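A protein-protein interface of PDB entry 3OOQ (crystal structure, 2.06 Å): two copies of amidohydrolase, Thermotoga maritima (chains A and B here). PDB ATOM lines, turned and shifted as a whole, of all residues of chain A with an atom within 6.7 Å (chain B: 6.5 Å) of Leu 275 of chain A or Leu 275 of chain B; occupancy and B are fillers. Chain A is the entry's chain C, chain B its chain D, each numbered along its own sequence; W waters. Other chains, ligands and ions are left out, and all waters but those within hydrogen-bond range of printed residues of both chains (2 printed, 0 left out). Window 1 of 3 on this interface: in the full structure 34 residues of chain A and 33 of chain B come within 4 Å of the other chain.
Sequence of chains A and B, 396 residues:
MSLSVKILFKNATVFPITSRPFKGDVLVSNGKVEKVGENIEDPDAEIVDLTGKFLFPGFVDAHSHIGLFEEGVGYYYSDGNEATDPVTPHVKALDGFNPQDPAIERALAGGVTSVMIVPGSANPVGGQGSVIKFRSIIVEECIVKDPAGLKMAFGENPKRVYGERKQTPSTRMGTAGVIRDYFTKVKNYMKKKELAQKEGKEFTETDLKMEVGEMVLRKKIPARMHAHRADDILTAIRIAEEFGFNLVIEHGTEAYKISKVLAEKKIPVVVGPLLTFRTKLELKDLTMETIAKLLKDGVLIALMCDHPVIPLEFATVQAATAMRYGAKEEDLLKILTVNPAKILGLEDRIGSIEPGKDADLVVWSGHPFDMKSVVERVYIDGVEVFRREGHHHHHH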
ATOM      1  N   GLY A 272     -16.426  -3.641   1.075  1.00  0.00           N
ATOM      2  CA  GLY A 272     -16.558  -4.779   1.973  1.00  0.00           C
ATOM      3  C   GLY A 272     -15.341  -4.779   2.873  1.00  0.00           C
ATOM      4  O   GLY A 272     -14.347  -4.103   2.575  1.00  0.00           O
ATOM      5  N   PRO A 273     -15.405  -5.516   3.997  1.00  0.00           N
ATOM      6  CA  PRO A 273     -16.568  -6.263   4.453  1.00  0.00           C
ATOM      7  C   PRO A 273     -17.691  -5.297   4.885  1.00  0.00           C
ATOM      8  O   PRO A 273     -17.423  -4.233   5.468  1.00  0.00           O
ATOM      9  CB  PRO A 273     -16.027  -7.051   5.650  1.00  0.00           C
ATOM     10  CG  PRO A 273     -14.886  -6.214   6.197  1.00  0.00           C
ATOM     11  CD  PRO A 273     -14.315  -5.473   5.001  1.00  0.00           C
ATOM     12  N   LEU A 274     -18.930  -5.658   4.568  1.00  0.00           N
ATOM     13  CA  LEU A 274     -20.084  -4.837   4.917  1.00  0.00           C
ATOM     14  C   LEU A 274     -21.033  -5.528   5.901  1.00  0.00           C
ATOM     15  O   LEU A 274     -21.594  -4.874   6.769  1.00  0.00           O
ATOM     16  CB  LEU A 274     -20.842  -4.417   3.649  1.00  0.00           C
ATOM     17  CG  LEU A 274     -20.130  -3.512   2.638  1.00  0.00           C
ATOM     18  CD1 LEU A 274     -20.896  -3.547   1.325  1.00  0.00           C
ATOM     19  CD2 LEU A 274     -19.991  -2.081   3.160  1.00  0.00           C
ATOM     20  N   LEU A 275     -21.230  -6.839   5.737  1.00  0.00           N
ATOM     21  CA  LEU A 275     -22.056  -7.637   6.646  1.00  0.00           C
ATOM     22  C   LEU A 275     -21.250  -7.917   7.908  1.00  0.00           C
ATOM     23  O   LEU A 275     -20.845  -9.062   8.160  1.00  0.00           O
ATOM     24  CB  LEU A 275     -22.474  -8.950   5.976  1.00  0.00           C
ATOM     25  CG  LEU A 275     -23.537  -9.804   6.684  1.00  0.00           C
ATOM     26  CD1 LEU A 275     -24.955  -9.264   6.438  1.00  0.00           C
ATOM     27  CD2 LEU A 275     -23.445 -11.243   6.222  1.00  0.00           C
ATOM     28  N   THR A 276     -20.996  -6.858   8.682  1.00  0.00           N
ATOM     29  CA  THR A 276     -19.988  -6.891   9.744  1.00  0.00           C
ATOM     30  C   THR A 276     -20.159  -5.739  10.740  1.00  0.00           C
ATOM     31  O   THR A 276     -20.725  -4.695  10.419  1.00  0.00           O
ATOM     32  CB  THR A 276     -18.528  -6.890   9.142  1.00  0.00           C
ATOM     33  OG1 THR A 276     -17.619  -7.543  10.048  1.00  0.00           O
ATOM     34  CG2 THR A 276     -18.034  -5.459   8.795  1.00  0.00           C
ATOM     35  N   PHE A 277     -19.670  -5.944  11.953  1.00  0.00           N
ATOM     36  CA  PHE A 277     -19.746  -4.961  13.017  1.00  0.00           C
ATOM     37  C   PHE A 277     -18.735  -3.837  12.796  1.00  0.00           C
ATOM     38  O   PHE A 277     -17.624  -4.083  12.326  1.00  0.00           O
ATOM     39  CB  PHE A 277     -19.475  -5.667  14.345  1.00  0.00           C
ATOM     40  CG  PHE A 277     -19.573  -4.779  15.563  1.00  0.00           C
ATOM     41  CD1 PHE A 277     -20.805  -4.406  16.075  1.00  0.00           C
ATOM     42  CD2 PHE A 277     -18.412  -4.393  16.251  1.00  0.00           C
ATOM     43  CE1 PHE A 277     -20.890  -3.616  17.232  1.00  0.00           C
ATOM     44  CE2 PHE A 277     -18.486  -3.593  17.404  1.00  0.00           C
ATOM     45  CZ  PHE A 277     -19.716  -3.204  17.890  1.00  0.00           C
ATOM     46  N   LEU A 286     -19.685   3.163   8.078  1.00  0.00           N
ATOM     47  CA  LEU A 286     -19.881   2.012   7.202  1.00  0.00           C
ATOM     48  C   LEU A 286     -21.369   1.840   6.920  1.00  0.00           C
ATOM     49  O   LEU A 286     -22.184   1.913   7.831  1.00  0.00           O
ATOM     50  CB  LEU A 286     -19.311   0.735   7.839  1.00  0.00           C
ATOM     51  CG  LEU A 286     -19.503  -0.586   7.076  1.00  0.00           C
ATOM     52  CD1 LEU A 286     -18.369  -1.557   7.294  1.00  0.00           C
ATOM     53  CD2 LEU A 286     -20.806  -1.248   7.477  1.00  0.00           C
ATOM     54  N   MET A 288     -24.135  -0.473   4.117  1.00  0.00           N
ATOM     55  CA  MET A 288     -24.396  -1.290   2.948  1.00  0.00           C
ATOM     56  C   MET A 288     -24.984  -0.508   1.767  1.00  0.00           C
ATOM     57  O   MET A 288     -24.916  -0.964   0.621  1.00  0.00           O
ATOM     58  CB  MET A 288     -25.248  -2.493   3.309  1.00  0.00           C
ATOM     59  CG  MET A 288     -24.726  -3.739   2.646  1.00  0.00           C
ATOM     60  SD  MET A 288     -25.277  -5.263   3.659  1.00  0.00           S
ATOM     61  CE  MET A 288     -23.796  -6.460   3.281  1.00  0.00           C
ATOM     62  N   VAL A 309     -12.825 -12.110   7.937  1.00  0.00           N
ATOM     63  CA  VAL A 309     -13.789 -11.221   8.643  1.00  0.00           C
ATOM     64  C   VAL A 309     -15.217 -11.737   8.417  1.00  0.00           C
ATOM     65  O   VAL A 309     -15.996 -11.894   9.370  1.00  0.00           O
ATOM     66  CB  VAL A 309     -13.650  -9.717   8.217  1.00  0.00           C
ATOM     67  CG1 VAL A 309     -14.679  -8.850   8.928  1.00  0.00           C
ATOM     68  CG2 VAL A 309     -12.272  -9.183   8.548  1.00  0.00           C
ATOM     69  N   ILE A 310     -15.532 -12.020   7.149  1.00  0.00           N
ATOM     70  CA  ILE A 310     -16.728 -12.782   6.774  1.00  0.00           C
ATOM     71  C   ILE A 310     -16.237 -14.010   6.018  1.00  0.00           C
ATOM     72  O   ILE A 310     -15.422 -13.864   5.096  1.00  0.00           O
ATOM     73  CB  ILE A 310     -17.656 -11.977   5.826  1.00  0.00           C
ATOM     74  CG1 ILE A 310     -18.070 -10.653   6.472  1.00  0.00           C
ATOM     75  CG2 ILE A 310     -18.892 -12.801   5.448  1.00  0.00           C
ATOM     76  CD1 ILE A 310     -18.648  -9.646   5.496  1.00  0.00           C
ATOM     77  N   PRO A 311     -16.728 -15.209   6.376  1.00  0.00           N
ATOM     78  CA  PRO A 311     -16.315 -16.378   5.614  1.00  0.00           C
ATOM     79  C   PRO A 311     -16.713 -16.313   4.140  1.00  0.00           C
ATOM     80  O   PRO A 311     -17.848 -15.923   3.788  1.00  0.00           O
ATOM     81  CB  PRO A 311     -17.030 -17.539   6.312  1.00  0.00           C
ATOM     82  CG  PRO A 311     -17.331 -17.048   7.666  1.00  0.00           C
ATOM     83  CD  PRO A 311     -17.585 -15.573   7.515  1.00  0.00           C
ATOM     84  N   PHE A 314     -19.894 -17.499   2.601  1.00  0.00           N
ATOM     85  CA  PHE A 314     -21.103 -16.677   2.711  1.00  0.00           C
ATOM     86  C   PHE A 314     -21.031 -15.420   1.841  1.00  0.00           C
ATOM     87  O   PHE A 314     -21.711 -14.417   2.118  1.00  0.00           O
ATOM     88  CB  PHE A 314     -21.413 -16.315   4.182  1.00  0.00           C
ATOM     89  CG  PHE A 314     -21.515 -17.515   5.114  1.00  0.00           C
ATOM     90  CD1 PHE A 314     -22.379 -18.570   4.832  1.00  0.00           C
ATOM     91  CD2 PHE A 314     -20.768 -17.557   6.300  1.00  0.00           C
ATOM     92  CE1 PHE A 314     -22.484 -19.655   5.687  1.00  0.00           C
ATOM     93  CE2 PHE A 314     -20.858 -18.638   7.175  1.00  0.00           C
ATOM     94  CZ  PHE A 314     -21.708 -19.704   6.868  1.00  0.00           C
ATOM     95  N   VAL A 317     -24.395 -14.487   0.721  1.00  0.00           N
ATOM     96  CA  VAL A 317     -25.212 -14.017   1.830  1.00  0.00           C
ATOM     97  C   VAL A 317     -25.027 -12.523   2.017  1.00  0.00           C
ATOM     98  O   VAL A 317     -26.014 -11.772   2.128  1.00  0.00           O
ATOM     99  CB  VAL A 317     -24.855 -14.747   3.132  1.00  0.00           C
ATOM    100  CG1 VAL A 317     -25.732 -14.255   4.307  1.00  0.00           C
ATOM    101  CG2 VAL A 317     -24.985 -16.254   2.917  1.00  0.00           C
ATOM    102  N   GLN A 318     -23.764 -12.097   2.047  1.00  0.00           N
ATOM    103  CA  GLN A 318     -23.454 -10.686   2.196  1.00  0.00           C
ATOM    104  C   GLN A 318     -24.068  -9.912   1.039  1.00  0.00           C
ATOM    105  O   GLN A 318     -24.680  -8.875   1.254  1.00  0.00           O
ATOM    106  CB  GLN A 318     -21.947 -10.427   2.247  1.00  0.00           C
ATOM    107  CG  GLN A 318     -21.606  -8.919   2.048  1.00  0.00           C
ATOM    108  CD  GLN A 318     -20.139  -8.589   2.283  1.00  0.00           C
ATOM    109  OE1 GLN A 318     -19.809  -7.788   3.157  1.00  0.00           O
ATOM    110  NE2 GLN A 318     -19.253  -9.229   1.527  1.00  0.00           N
ATOM    111  N   ALA A 319     -23.901 -10.432  -0.179  1.00  0.00           N
ATOM    112  CA  ALA A 319     -24.387  -9.753  -1.377  1.00  0.00           C
ATOM    113  C   ALA A 319     -25.910  -9.639  -1.389  1.00  0.00           C
ATOM    114  O   ALA A 319     -26.443  -8.555  -1.635  1.00  0.00           O
ATOM    115  CB  ALA A 319     -23.877 -10.435  -2.646  1.00  0.00           C
ATOM    116  N   THR A 321     -27.977  -9.647   1.022  1.00  0.00           N
ATOM    117  CA  THR A 321     -28.383  -8.776   2.105  1.00  0.00           C
ATOM    118  C   THR A 321     -28.381  -7.298   1.716  1.00  0.00           C
ATOM    119  O   THR A 321     -29.166  -6.524   2.251  1.00  0.00           O
ATOM    120  CB  THR A 321     -27.498  -9.014   3.337  1.00  0.00           C
ATOM    121  OG1 THR A 321     -27.754 -10.329   3.825  1.00  0.00           O
ATOM    122  CG2 THR A 321     -27.789  -8.013   4.446  1.00  0.00           C
ATOM    123  N   ALA A 322     -27.511  -6.918   0.786  1.00  0.00           N
ATOM    124  CA  ALA A 322     -27.480  -5.543   0.271  1.00  0.00           C
ATOM    125  C   ALA A 322     -28.780  -5.150  -0.449  1.00  0.00           C
ATOM    126  O   ALA A 322     -29.056  -3.966  -0.617  1.00  0.00           O
ATOM    127  CB  ALA A 322     -26.268  -5.325  -0.659  1.00  0.00           C
ATOM    128  N   GLY B 272     -25.163 -20.622  18.222  1.00  0.00           N
ATOM    129  CA  GLY B 272     -24.677 -19.382  17.628  1.00  0.00           C
ATOM    130  C   GLY B 272     -23.503 -18.863  18.437  1.00  0.00           C
ATOM    131  O   GLY B 272     -23.301 -19.289  19.573  1.00  0.00           O
ATOM    132  N   PRO B 273     -22.705 -17.964  17.849  1.00  0.00           N
ATOM    133  CA  PRO B 273     -22.884 -17.530  16.453  1.00  0.00           C
ATOM    134  C   PRO B 273     -22.487 -18.639  15.440  1.00  0.00           C
ATOM    135  O   PRO B 273     -21.555 -19.403  15.686  1.00  0.00           O
ATOM    136  CB  PRO B 273     -21.951 -16.317  16.348  1.00  0.00           C
ATOM    137  CG  PRO B 273     -20.815 -16.613  17.353  1.00  0.00           C
ATOM    138  CD  PRO B 273     -21.412 -17.535  18.421  1.00  0.00           C
ATOM    139  N   LEU B 274     -23.208 -18.721  14.325  1.00  0.00           N
ATOM    140  CA  LEU B 274     -22.985 -19.728  13.300  1.00  0.00           C
ATOM    141  C   LEU B 274     -22.549 -19.147  11.958  1.00  0.00           C
ATOM    142  O   LEU B 274     -21.782 -19.779  11.246  1.00  0.00           O
ATOM    143  CB  LEU B 274     -24.227 -20.621  13.115  1.00  0.00           C
ATOM    144  CG  LEU B 274     -24.719 -21.406  14.344  1.00  0.00           C
ATOM    145  CD1 LEU B 274     -26.143 -21.895  14.104  1.00  0.00           C
ATOM    146  CD2 LEU B 274     -23.801 -22.585  14.679  1.00  0.00           C
ATOM    147  N   LEU B 275     -23.033 -17.949  11.624  1.00  0.00           N
ATOM    148  CA  LEU B 275     -22.644 -17.268  10.379  1.00  0.00           C
ATOM    149  C   LEU B 275     -21.335 -16.540  10.628  1.00  0.00           C
ATOM    150  O   LEU B 275     -21.303 -15.314  10.632  1.00  0.00           O
ATOM    151  CB  LEU B 275     -23.708 -16.242   9.976  1.00  0.00           C
ATOM    152  CG  LEU B 275     -23.584 -15.603   8.584  1.00  0.00           C
ATOM    153  CD1 LEU B 275     -24.054 -16.559   7.490  1.00  0.00           C
ATOM    154  CD2 LEU B 275     -24.379 -14.294   8.538  1.00  0.00           C
ATOM    155  N   THR B 276     -20.259 -17.293  10.831  1.00  0.00           N
ATOM    156  CA  THR B 276     -19.009 -16.726  11.365  1.00  0.00           C
ATOM    157  C   THR B 276     -17.823 -17.668  11.143  1.00  0.00           C
ATOM    158  O   THR B 276     -18.017 -18.857  10.886  1.00  0.00           O
ATOM    159  CB  THR B 276     -19.176 -16.367  12.868  1.00  0.00           C
ATOM    160  OG1 THR B 276     -18.221 -15.364  13.258  1.00  0.00           O
ATOM    161  CG2 THR B 276     -19.076 -17.595  13.763  1.00  0.00           C
ATOM    162  N   PHE B 277     -16.603 -17.122  11.207  1.00  0.00           N
ATOM    163  CA  PHE B 277     -15.367 -17.865  10.942  1.00  0.00           C
ATOM    164  C   PHE B 277     -14.982 -18.701  12.164  1.00  0.00           C
ATOM    165  O   PHE B 277     -15.156 -18.266  13.301  1.00  0.00           O
ATOM    166  CB  PHE B 277     -14.236 -16.884  10.606  1.00  0.00           C
ATOM    167  CG  PHE B 277     -12.927 -17.547  10.208  1.00  0.00           C
ATOM    168  CD1 PHE B 277     -12.809 -18.222   8.996  1.00  0.00           C
ATOM    169  CD2 PHE B 277     -11.812 -17.466  11.038  1.00  0.00           C
ATOM    170  CE1 PHE B 277     -11.609 -18.816   8.620  1.00  0.00           C
ATOM    171  CE2 PHE B 277     -10.588 -18.053  10.664  1.00  0.00           C
ATOM    172  CZ  PHE B 277     -10.491 -18.725   9.460  1.00  0.00           C
ATOM    173  N   LEU B 286     -17.695 -26.466  14.309  1.00  0.00           N
ATOM    174  CA  LEU B 286     -18.873 -25.641  14.149  1.00  0.00           C
ATOM    175  C   LEU B 286     -19.545 -25.951  12.795  1.00  0.00           C
ATOM    176  O   LEU B 286     -18.871 -26.070  11.759  1.00  0.00           O
ATOM    177  CB  LEU B 286     -18.503 -24.152  14.228  1.00  0.00           C
ATOM    178  CG  LEU B 286     -19.622 -23.108  14.143  1.00  0.00           C
ATOM    179  CD1 LEU B 286     -19.233 -21.848  14.871  1.00  0.00           C
ATOM    180  CD2 LEU B 286     -19.915 -22.761  12.695  1.00  0.00           C
ATOM    181  N   MET B 288     -23.542 -25.132  10.669  1.00  0.00           N
ATOM    182  CA  MET B 288     -24.918 -24.665  10.653  1.00  0.00           C
ATOM    183  C   MET B 288     -25.919 -25.825  10.652  1.00  0.00           C
ATOM    184  O   MET B 288     -27.094 -25.629  10.962  1.00  0.00           O
ATOM    185  CB  MET B 288     -25.152 -23.705   9.495  1.00  0.00           C
ATOM    186  CG  MET B 288     -25.993 -22.522   9.915  1.00  0.00           C
ATOM    187  SD  MET B 288     -25.618 -21.014   8.794  1.00  0.00           S
ATOM    188  CE  MET B 288     -26.097 -19.630  10.048  1.00  0.00           C
ATOM    189  N   VAL B 309     -20.182 -10.246  17.506  1.00  0.00           N
ATOM    190  CA  VAL B 309     -19.592 -11.221  16.574  1.00  0.00           C
ATOM    191  C   VAL B 309     -20.403 -11.237  15.260  1.00  0.00           C
ATOM    192  O   VAL B 309     -19.844 -11.190  14.158  1.00  0.00           O
ATOM    193  CB  VAL B 309     -19.453 -12.633  17.183  1.00  0.00           C
ATOM    194  CG1 VAL B 309     -18.819 -13.576  16.167  1.00  0.00           C
ATOM    195  CG2 VAL B 309     -18.596 -12.605  18.466  1.00  0.00           C
ATOM    196  N   ILE B 310     -21.722 -11.286  15.387  1.00  0.00           N
ATOM    197  CA  ILE B 310     -22.592 -10.985  14.264  1.00  0.00           C
ATOM    198  C   ILE B 310     -23.473  -9.808  14.668  1.00  0.00           C
ATOM    199  O   ILE B 310     -24.076  -9.836  15.734  1.00  0.00           O
ATOM    200  CB  ILE B 310     -23.457 -12.199  13.858  1.00  0.00           C
ATOM    201  CG1 ILE B 310     -22.551 -13.392  13.520  1.00  0.00           C
ATOM    202  CG2 ILE B 310     -24.372 -11.855  12.677  1.00  0.00           C
ATOM    203  CD1 ILE B 310     -23.300 -14.693  13.422  1.00  0.00           C
ATOM    204  N   PRO B 311     -23.548  -8.760  13.825  1.00  0.00           N
ATOM    205  CA  PRO B 311     -24.423  -7.663  14.219  1.00  0.00           C
ATOM    206  C   PRO B 311     -25.872  -8.120  14.360  1.00  0.00           C
ATOM    207  O   PRO B 311     -26.400  -8.854  13.523  1.00  0.00           O
ATOM    208  CB  PRO B 311     -24.266  -6.658  13.075  1.00  0.00           C
ATOM    209  CG  PRO B 311     -22.902  -6.937  12.531  1.00  0.00           C
ATOM    210  CD  PRO B 311     -22.715  -8.420  12.658  1.00  0.00           C
ATOM    211  N   PHE B 314     -28.555  -8.221  11.740  1.00  0.00           N
ATOM    212  CA  PHE B 314     -28.514  -9.310  10.755  1.00  0.00           C
ATOM    213  C   PHE B 314     -28.920 -10.650  11.348  1.00  0.00           C
ATOM    214  O   PHE B 314     -28.590 -11.698  10.801  1.00  0.00           O
ATOM    215  CB  PHE B 314     -27.123  -9.433  10.092  1.00  0.00           C
ATOM    216  CG  PHE B 314     -26.622  -8.152   9.453  1.00  0.00           C
ATOM    217  CD1 PHE B 314     -27.427  -7.422   8.589  1.00  0.00           C
ATOM    218  CD2 PHE B 314     -25.328  -7.704   9.697  1.00  0.00           C
ATOM    219  CE1 PHE B 314     -26.963  -6.245   7.987  1.00  0.00           C
ATOM    220  CE2 PHE B 314     -24.853  -6.533   9.110  1.00  0.00           C
ATOM    221  CZ  PHE B 314     -25.674  -5.801   8.238  1.00  0.00           C
ATOM    222  N   VAL B 317     -30.735 -12.547   8.752  1.00  0.00           N
ATOM    223  CA  VAL B 317     -29.766 -13.039   7.755  1.00  0.00           C
ATOM    224  C   VAL B 317     -29.120 -14.378   8.194  1.00  0.00           C
ATOM    225  O   VAL B 317     -29.074 -15.345   7.421  1.00  0.00           O
ATOM    226  CB  VAL B 317     -28.684 -11.980   7.450  1.00  0.00           C
ATOM    227  CG1 VAL B 317     -27.728 -12.474   6.393  1.00  0.00           C
ATOM    228  CG2 VAL B 317     -29.338 -10.668   6.977  1.00  0.00           C
ATOM    229  N   GLN B 318     -28.634 -14.434   9.426  1.00  0.00           N
ATOM    230  CA  GLN B 318     -28.055 -15.682   9.954  1.00  0.00           C
ATOM    231  C   GLN B 318     -29.088 -16.801   9.928  1.00  0.00           C
ATOM    232  O   GLN B 318     -28.809 -17.904   9.457  1.00  0.00           O
ATOM    233  CB  GLN B 318     -27.563 -15.517  11.393  1.00  0.00           C
ATOM    234  CG  GLN B 318     -27.067 -16.839  11.978  1.00  0.00           C
ATOM    235  CD  GLN B 318     -26.368 -16.708  13.314  1.00  0.00           C
ATOM    236  OE1 GLN B 318     -25.295 -17.270  13.510  1.00  0.00           O
ATOM    237  NE2 GLN B 318     -26.978 -15.989  14.243  1.00  0.00           N
ATOM    238  N   THR B 321     -30.030 -18.058   6.415  1.00  0.00           N
ATOM    239  CA  THR B 321     -28.931 -18.806   5.802  1.00  0.00           C
ATOM    240  C   THR B 321     -28.945 -20.272   6.225  1.00  0.00           C
ATOM    241  O   THR B 321     -28.541 -21.152   5.460  1.00  0.00           O
ATOM    242  CB  THR B 321     -27.566 -18.150   6.117  1.00  0.00           C
ATOM    243  OG1 THR B 321     -27.568 -16.814   5.592  1.00  0.00           O
ATOM    244  CG2 THR B 321     -26.396 -18.950   5.498  1.00  0.00           C
HETATM  245  O   HOH W   1     -18.975  -8.816  13.063  1.00  0.00           O
HETATM  246  O   HOH W   2     -16.398 -14.298  10.825  1.00  0.00           O
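Water W1 lies within hydrogen-bond range of O of Val 309 of chain B and N of Phe 277 of chain A. Water W2 lies within hydrogen-bond range of the backbone carbonyl oxygen (O) of Val 309 of chain A (2.8 Å), the backbone NH (N) of Phe 277 of chain B (2.9 Å) and the side-chain hydroxyl (OG1) of Thr 276 of chain B (3.2 Å).
Of the printed residues of chain B, Pro 311 of chain A touches Thr 276 and Phe 277. Printed residues of chain B within 4 Å of Val 317 of chain A: Val 317 (3.4 Å) and Thr 321 (3.4 Å). Leu 275 of chain B touches two residues of chain A. The nearest residue of chain A that does not touch Leu 275 of chain B is Val 317 of chain A (4.3 Å). The nearest printed residue of chain B that does not touch Thr 276 of chain A is Val 309 of chain B (5.9 Å).
Leu 275 of chain A touches Phe 314 of chain B, and with the chains exchanged Phe 314 of chain A touches Leu 275 of chain B. Thr 276 of chain A touches Phe 314 of chain B, and with the chains exchanged Phe 314 of chain A touches Thr 276 of chain B. Phe 277 of chain A touches Pro 311 of chain B, and with the chains exchanged Pro 311 of chain A touches Phe 277 of chain B. Phe 314 of chain A touches Thr 321 of chain B, but with the chains exchanged Thr 321 of chain A does not touch Phe 314 of chain B (4.04 Å). Positions printed for both chains: 272, 273, 274, 275, 276, 277, 286, 288, 309, 310, 311, 314, 317, 318 and 321. Of the 13 pairs that touch across the chains among the printed residues, 12 have their exchanged pair printed and touching as well.
Of the 15 printed residues of chain B, 7 touch a printed residue of chain A. Of the 17 printed residues of chain A, 7 touch a printed residue of chain B. Hydrophobic or aromatic side chains of chain A within 4 Å of the printed part of chain B: Leu 275, Pro 311, Phe 314 and Val 317. Along chain A the printed residues that touch a printed residue of chain B span positions 275 to 321.
Among the printed residues, merely in contact across the chains: Leu 275 of chain A with Leu 275 of chain B (3.9 Å), Leu 275 of chain A with Phe 314 of chain B (3.6 Å), Thr 276 of chain A with Pro 311 of chain B (3.5 Å), Thr 276 of chain A with Phe 314 of chain B (3.9 Å), Phe 277 of chain A with Pro 311 of chain B (3.4 Å), Pro 311 of chain A with Thr 276 of chain B (3.6 Å), Pro 311 of chain A with Phe 277 of chain B (3.6 Å), Phe 314 of chain A with Leu 275 of chain B (3.6 Å), Phe 314 of chain A with Thr 276 of chain B (3.9 Å), Phe 314 of chain A with Thr 321 of chain B (3.98 Å), Val 317 of chain A with Val 317 of chain B (3.4 Å), Val 317 of chain A with Thr 321 of chain B (3.4 Å) and Thr 321 of chain A with Val 317 of chain B (3.3 Å).
N of Leu 275 of chain A lies within hydrogen-bond range of OE1 of Gln 318 of chain A (3.1 Å). O of Val 317 of chain A is in hydrogen-bond range of OG1 of Thr 321 of chain A, at 2.8 Å. The side-chain amide oxygen (OE1) of Gln 318 of chain B is in hydrogen-bond range of the backbone NH (N) of Leu 275 of chain B (3.0 Å). OG1 of Thr 321 of chain B lies within hydrogen-bond range of O of Val 317 of chain B (2.8 Å).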
